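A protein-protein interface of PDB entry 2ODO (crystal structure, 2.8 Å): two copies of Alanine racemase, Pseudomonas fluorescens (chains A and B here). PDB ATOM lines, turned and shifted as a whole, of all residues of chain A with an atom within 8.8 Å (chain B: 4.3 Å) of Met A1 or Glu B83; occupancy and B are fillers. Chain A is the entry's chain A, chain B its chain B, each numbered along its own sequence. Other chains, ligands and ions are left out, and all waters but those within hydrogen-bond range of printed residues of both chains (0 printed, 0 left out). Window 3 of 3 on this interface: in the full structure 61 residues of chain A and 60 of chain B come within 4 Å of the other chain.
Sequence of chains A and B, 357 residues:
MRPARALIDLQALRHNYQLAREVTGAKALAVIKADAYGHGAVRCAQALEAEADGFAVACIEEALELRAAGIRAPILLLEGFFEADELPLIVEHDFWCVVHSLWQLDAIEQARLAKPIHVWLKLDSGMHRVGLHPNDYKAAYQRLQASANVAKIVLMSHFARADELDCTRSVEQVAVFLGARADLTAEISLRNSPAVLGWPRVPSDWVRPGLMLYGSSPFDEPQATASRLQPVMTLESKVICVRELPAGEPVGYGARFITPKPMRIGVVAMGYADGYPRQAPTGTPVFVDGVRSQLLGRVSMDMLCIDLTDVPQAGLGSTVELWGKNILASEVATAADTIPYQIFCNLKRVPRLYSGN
No position is printed for both chains.
Of the 10 pairs that touch across the chains among the printed residues, none has its exchanged pair printed and touching as well.
O of Ala A269 is in hydrogen-bond range of OG of Ser A237, at 2.7 Å.
The backbone NH of Ala A269 is in hydrogen-bond range of the backbone carbonyl oxygen of Lys A238, at 3.2 Å.
The backbone NH (N) of Phe B82 lies within hydrogen-bond range of the side-chain carboxylate (OE2) of Glu B86, 3.0 Å away.
The backbone NH (N) of Glu B83 sits at hydrogen-bond distance from the side-chain carboxylate (OE2) of Glu B86 (2.8 Å).
Of chain B, only Ile B60 (3.9 Å), Glu B61 (3.3 Å), Phe B82 (3.4 Å), Glu B83 (2.8 Å) and Glu B86 (2.8 Å) come within 4 Å of Met A1.
Printed residues of chain B within 4 Å of Ile A240: Phe B82.
Of the printed residues of chain A, Glu B61 touches Met A1 (3.3 Å) and Arg A2 (3.3 Å).
Printed residues of chain A within 4 Å of Phe B82: Met A1 (3.4 Å), Arg A2 (3.7 Å), Pro A3 (3.7 Å), Ile A240 (3.8 Å) and Ala A269 (3.95 Å).
Of chain A, only Met A1 (2.8 Å) comes within 4 Å of Glu B83.
No residue of chain A comes within 4 Å of Ala B84.
The nearest residue of chain A that does not touch Glu B83 is Lys A238 (5.3 Å).
Printed residues of chain A that touch a printed residue of chain B: Met A1, Arg A2, Pro A3, Ile A240 and Ala A269.
Of the 8 printed residues of chain B, 5 touch a printed residue of chain A.
Among the printed residues, no Asp or Glu carboxylate lies within 4 Å of a Lys or Arg side-chain nitrogen of the other chain.
Among the printed residues, pairs that only touch across the chains: Met A1 with Ile B60, Met A1 with Glu B61, Met A1 with Phe B82, Arg A2 with Phe B82, Pro A3 with Phe B82, Ile A240 with Phe B82 and Ala A269 with Phe B82.
The backbone NH (N) of Met A1 sits at hydrogen-bond distance from the side-chain carboxylate (OE1) of Glu B83 (2.8 Å).
N of Met A1 is in hydrogen-bond range of OE2 of Glu B86.
The backbone NH (N) of Arg A2 sits at hydrogen-bond distance from the side-chain carboxylate (OE1) of Glu B61 (3.3 Å).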
ATOM      1  N   MET A   1      -9.358  16.882  32.236  1.00  0.00           N
ATOM      2  CA  MET A   1     -10.404  15.819  32.151  1.00  0.00           C
ATOM      3  C   MET A   1     -11.559  16.265  31.256  1.00  0.00           C
ATOM      4  O   MET A   1     -11.627  17.432  30.860  1.00  0.00           O
ATOM      5  CB  MET A   1     -10.925  15.455  33.549  1.00  0.00           C
ATOM      6  CG  MET A   1      -9.844  15.253  34.611  1.00  0.00           C
ATOM      7  SD  MET A   1      -8.558  14.064  34.168  1.00  0.00           S
ATOM      8  CE  MET A   1      -9.452  12.515  34.262  1.00  0.00           C
ATOM      9  N   ARG A   2     -12.454  15.331  30.937  1.00  0.00           N
ATOM     10  CA  ARG A   2     -13.643  15.626  30.137  1.00  0.00           C
ATOM     11  C   ARG A   2     -14.582  16.551  30.916  1.00  0.00           C
ATOM     12  O   ARG A   2     -15.004  16.211  32.025  1.00  0.00           O
ATOM     13  CB  ARG A   2     -14.354  14.328  29.736  1.00  0.00           C
ATOM     14  CG  ARG A   2     -15.409  14.485  28.648  1.00  0.00           C
ATOM     15  CD  ARG A   2     -15.755  13.145  28.026  1.00  0.00           C
ATOM     16  NE  ARG A   2     -16.848  13.246  27.061  1.00  0.00           N
ATOM     17  CZ  ARG A   2     -18.077  12.773  27.256  1.00  0.00           C
ATOM     18  NH1 ARG A   2     -18.392  12.149  28.385  1.00  0.00           N
ATOM     19  NH2 ARG A   2     -18.997  12.918  26.312  1.00  0.00           N
ATOM     20  N   PRO A   3     -14.907  17.725  30.340  1.00  0.00           N
ATOM     21  CA  PRO A   3     -15.654  18.776  31.045  1.00  0.00           C
ATOM     22  C   PRO A   3     -17.090  18.399  31.426  1.00  0.00           C
ATOM     23  O   PRO A   3     -17.719  19.108  32.216  1.00  0.00           O
ATOM     24  CB  PRO A   3     -15.649  19.940  30.047  1.00  0.00           C
ATOM     25  CG  PRO A   3     -15.455  19.309  28.722  1.00  0.00           C
ATOM     26  CD  PRO A   3     -14.570  18.128  28.961  1.00  0.00           C
ATOM     27  N   ALA A   4     -17.589  17.295  30.877  1.00  0.00           N
ATOM     28  CA  ALA A   4     -18.949  16.828  31.140  1.00  0.00           C
ATOM     29  C   ALA A   4     -19.151  16.427  32.601  1.00  0.00           C
ATOM     30  O   ALA A   4     -18.383  15.635  33.152  1.00  0.00           O
ATOM     31  CB  ALA A   4     -19.299  15.676  30.215  1.00  0.00           C
ATOM     32  N   SER A 237     -21.722  20.698  30.113  1.00  0.00           N
ATOM     33  CA  SER A 237     -20.419  20.411  29.518  1.00  0.00           C
ATOM     34  C   SER A 237     -19.854  21.683  28.875  1.00  0.00           C
ATOM     35  O   SER A 237     -20.384  22.776  29.089  1.00  0.00           O
ATOM     36  CB  SER A 237     -20.533  19.275  28.496  1.00  0.00           C
ATOM     37  OG  SER A 237     -19.253  18.825  28.091  1.00  0.00           O
ATOM     38  N   LYS A 238     -18.782  21.544  28.098  1.00  0.00           N
ATOM     39  CA  LYS A 238     -18.119  22.704  27.498  1.00  0.00           C
ATOM     40  C   LYS A 238     -17.888  22.572  25.997  1.00  0.00           C
ATOM     41  O   LYS A 238     -17.878  21.466  25.450  1.00  0.00           O
ATOM     42  CB  LYS A 238     -16.787  22.989  28.201  1.00  0.00           C
ATOM     43  CG  LYS A 238     -16.917  23.633  29.571  1.00  0.00           C
ATOM     44  CD  LYS A 238     -15.561  23.770  30.232  1.00  0.00           C
ATOM     45  CE  LYS A 238     -15.673  24.405  31.606  1.00  0.00           C
ATOM     46  NZ  LYS A 238     -14.355  24.419  32.297  1.00  0.00           N
ATOM     47  N   ILE A 240     -15.586  22.419  22.973  1.00  0.00           N
ATOM     48  CA  ILE A 240     -14.219  21.940  22.766  1.00  0.00           C
ATOM     49  C   ILE A 240     -13.689  22.259  21.365  1.00  0.00           C
ATOM     50  O   ILE A 240     -12.512  22.037  21.073  1.00  0.00           O
ATOM     51  CB  ILE A 240     -14.099  20.416  23.039  1.00  0.00           C
ATOM     52  CG1 ILE A 240     -15.019  19.618  22.101  1.00  0.00           C
ATOM     53  CG2 ILE A 240     -14.392  20.115  24.512  1.00  0.00           C
ATOM     54  CD1 ILE A 240     -14.768  18.118  22.087  1.00  0.00           C
ATOM     55  N   ALA A 269     -18.700  18.537  24.354  1.00  0.00           N
ATOM     56  CA  ALA A 269     -18.329  17.225  24.877  1.00  0.00           C
ATOM     57  C   ALA A 269     -19.504  16.549  25.596  1.00  0.00           C
ATOM     58  O   ALA A 269     -19.534  16.482  26.827  1.00  0.00           O
ATOM     59  CB  ALA A 269     -17.120  17.344  25.800  1.00  0.00           C
ATOM     60  N   GLY A 317     -14.235  26.715  25.781  1.00  0.00           N
ATOM     61  CA  GLY A 317     -14.314  26.693  27.240  1.00  0.00           C
ATOM     62  C   GLY A 317     -15.609  27.227  27.831  1.00  0.00           C
ATOM     63  O   GLY A 317     -15.756  27.276  29.054  1.00  0.00           O
ATOM     64  N   PRO A 351     -19.519  12.000  35.629  1.00  0.00           N
ATOM     65  CA  PRO A 351     -19.465  12.008  37.089  1.00  0.00           C
ATOM     66  C   PRO A 351     -20.602  12.825  37.703  1.00  0.00           C
ATOM     67  O   PRO A 351     -20.870  13.946  37.261  1.00  0.00           O
ATOM     68  CB  PRO A 351     -18.111  12.663  37.386  1.00  0.00           C
ATOM     69  CG  PRO A 351     -17.816  13.495  36.193  1.00  0.00           C
ATOM     70  CD  PRO A 351     -18.409  12.764  35.028  1.00  0.00           C
ATOM     71  N   ILE B  60      -9.781  10.501  28.133  1.00  0.00           N
ATOM     72  CA  ILE B  60      -8.677  10.015  28.965  1.00  0.00           C
ATOM     73  C   ILE B  60      -9.132   9.086  30.103  1.00  0.00           C
ATOM     74  O   ILE B  60      -8.457   8.100  30.402  1.00  0.00           O
ATOM     75  CB  ILE B  60      -7.781  11.192  29.486  1.00  0.00           C
ATOM     76  CG1 ILE B  60      -6.460  10.665  30.064  1.00  0.00           C
ATOM     77  CG2 ILE B  60      -8.541  12.085  30.474  1.00  0.00           C
ATOM     78  CD1 ILE B  60      -5.333  11.687  30.084  1.00  0.00           C
ATOM     79  N   GLU B  61     -10.279   9.383  30.714  1.00  0.00           N
ATOM     80  CA  GLU B  61     -10.808   8.551  31.802  1.00  0.00           C
ATOM     81  C   GLU B  61     -11.187   7.136  31.359  1.00  0.00           C
ATOM     82  O   GLU B  61     -11.071   6.189  32.138  1.00  0.00           O
ATOM     83  CB  GLU B  61     -11.966   9.233  32.558  1.00  0.00           C
ATOM     84  CG  GLU B  61     -12.860  10.152  31.733  1.00  0.00           C
ATOM     85  CD  GLU B  61     -12.399  11.603  31.747  1.00  0.00           C
ATOM     86  OE1 GLU B  61     -11.980  12.107  30.684  1.00  0.00           O
ATOM     87  OE2 GLU B  61     -12.454  12.242  32.821  1.00  0.00           O
ATOM     88  N   PHE B  81      -6.888  15.424  24.209  1.00  0.00           N
ATOM     89  CA  PHE B  81      -7.034  15.989  25.549  1.00  0.00           C
ATOM     90  C   PHE B  81      -8.012  17.162  25.564  1.00  0.00           C
ATOM     91  O   PHE B  81      -8.077  17.942  24.611  1.00  0.00           O
ATOM     92  CB  PHE B  81      -5.672  16.395  26.135  1.00  0.00           C
ATOM     93  CG  PHE B  81      -4.918  17.401  25.306  1.00  0.00           C
ATOM     94  CD1 PHE B  81      -5.048  18.764  25.554  1.00  0.00           C
ATOM     95  CD2 PHE B  81      -4.065  16.986  24.291  1.00  0.00           C
ATOM     96  CE1 PHE B  81      -4.350  19.697  24.793  1.00  0.00           C
ATOM     97  CE2 PHE B  81      -3.365  17.910  23.525  1.00  0.00           C
ATOM     98  CZ  PHE B  81      -3.507  19.268  23.778  1.00  0.00           C
ATOM     99  N   PHE B  82      -8.770  17.273  26.652  1.00  0.00           N
ATOM    100  CA  PHE B  82      -9.737  18.354  26.826  1.00  0.00           C
ATOM    101  C   PHE B  82      -9.103  19.536  27.547  1.00  0.00           C
ATOM    102  O   PHE B  82      -9.387  20.691  27.232  1.00  0.00           O
ATOM    103  CB  PHE B  82     -10.974  17.861  27.583  1.00  0.00           C
ATOM    104  CG  PHE B  82     -11.723  16.763  26.875  1.00  0.00           C
ATOM    105  CD1 PHE B  82     -12.721  17.067  25.955  1.00  0.00           C
ATOM    106  CD2 PHE B  82     -11.428  15.427  27.127  1.00  0.00           C
ATOM    107  CE1 PHE B  82     -13.415  16.057  25.297  1.00  0.00           C
ATOM    108  CE2 PHE B  82     -12.116  14.412  26.474  1.00  0.00           C
ATOM    109  CZ  PHE B  82     -13.113  14.727  25.559  1.00  0.00           C
ATOM    110  N   GLU B  83      -8.242  19.234  28.517  1.00  0.00           N
ATOM    111  CA  GLU B  83      -7.463  20.249  29.224  1.00  0.00           C
ATOM    112  C   GLU B  83      -5.971  20.010  29.008  1.00  0.00           C
ATOM    113  O   GLU B  83      -5.538  18.867  28.836  1.00  0.00           O
ATOM    114  CB  GLU B  83      -7.804  20.252  30.718  1.00  0.00           C
ATOM    115  CG  GLU B  83      -9.177  20.834  31.041  1.00  0.00           C
ATOM    116  CD  GLU B  83      -9.558  20.688  32.505  1.00  0.00           C
ATOM    117  OE1 GLU B  83      -9.493  19.558  33.035  1.00  0.00           O
ATOM    118  OE2 GLU B  83      -9.937  21.706  33.124  1.00  0.00           O
ATOM    119  N   ALA B  84      -5.197  21.095  29.019  1.00  0.00           N
ATOM    120  CA  ALA B  84      -3.753  21.051  28.757  1.00  0.00           C
ATOM    121  C   ALA B  84      -2.968  20.163  29.728  1.00  0.00           C
ATOM    122  O   ALA B  84      -2.028  19.476  29.320  1.00  0.00           O
ATOM    123  CB  ALA B  84      -3.174  22.464  28.739  1.00  0.00           C
ATOM    124  N   ASP B  85      -3.361  20.172  31.001  1.00  0.00           N
ATOM    125  CA  ASP B  85      -2.669  19.396  32.034  1.00  0.00           C
ATOM    126  C   ASP B  85      -3.016  17.898  32.038  1.00  0.00           C
ATOM    127  O   ASP B  85      -2.748  17.191  33.014  1.00  0.00           O
ATOM    128  CB  ASP B  85      -2.863  20.024  33.426  1.00  0.00           C
ATOM    129  CG  ASP B  85      -4.324  20.250  33.775  1.00  0.00           C
ATOM    130  OD1 ASP B  85      -4.804  19.620  34.742  1.00  0.00           O
ATOM    131  OD2 ASP B  85      -4.987  21.057  33.087  1.00  0.00           O
ATOM    132  N   GLU B  86      -3.604  17.422  30.943  1.00  0.00           N
ATOM    133  CA  GLU B  86      -3.808  15.989  30.726  1.00  0.00           C
ATOM    134  C   GLU B  86      -2.564  15.363  30.100  1.00  0.00           C
ATOM    135  O   GLU B  86      -2.374  14.148  30.163  1.00  0.00           O
ATOM    136  CB  GLU B  86      -5.017  15.738  29.822  1.00  0.00           C
ATOM    137  CG  GLU B  86      -6.371  15.958  30.485  1.00  0.00           C
ATOM    138  CD  GLU B  86      -7.535  15.817  29.514  1.00  0.00           C
ATOM    139  OE1 GLU B  86      -7.549  14.853  28.719  1.00  0.00           O
ATOM    140  OE2 GLU B  86      -8.443  16.675  29.550  1.00  0.00           O
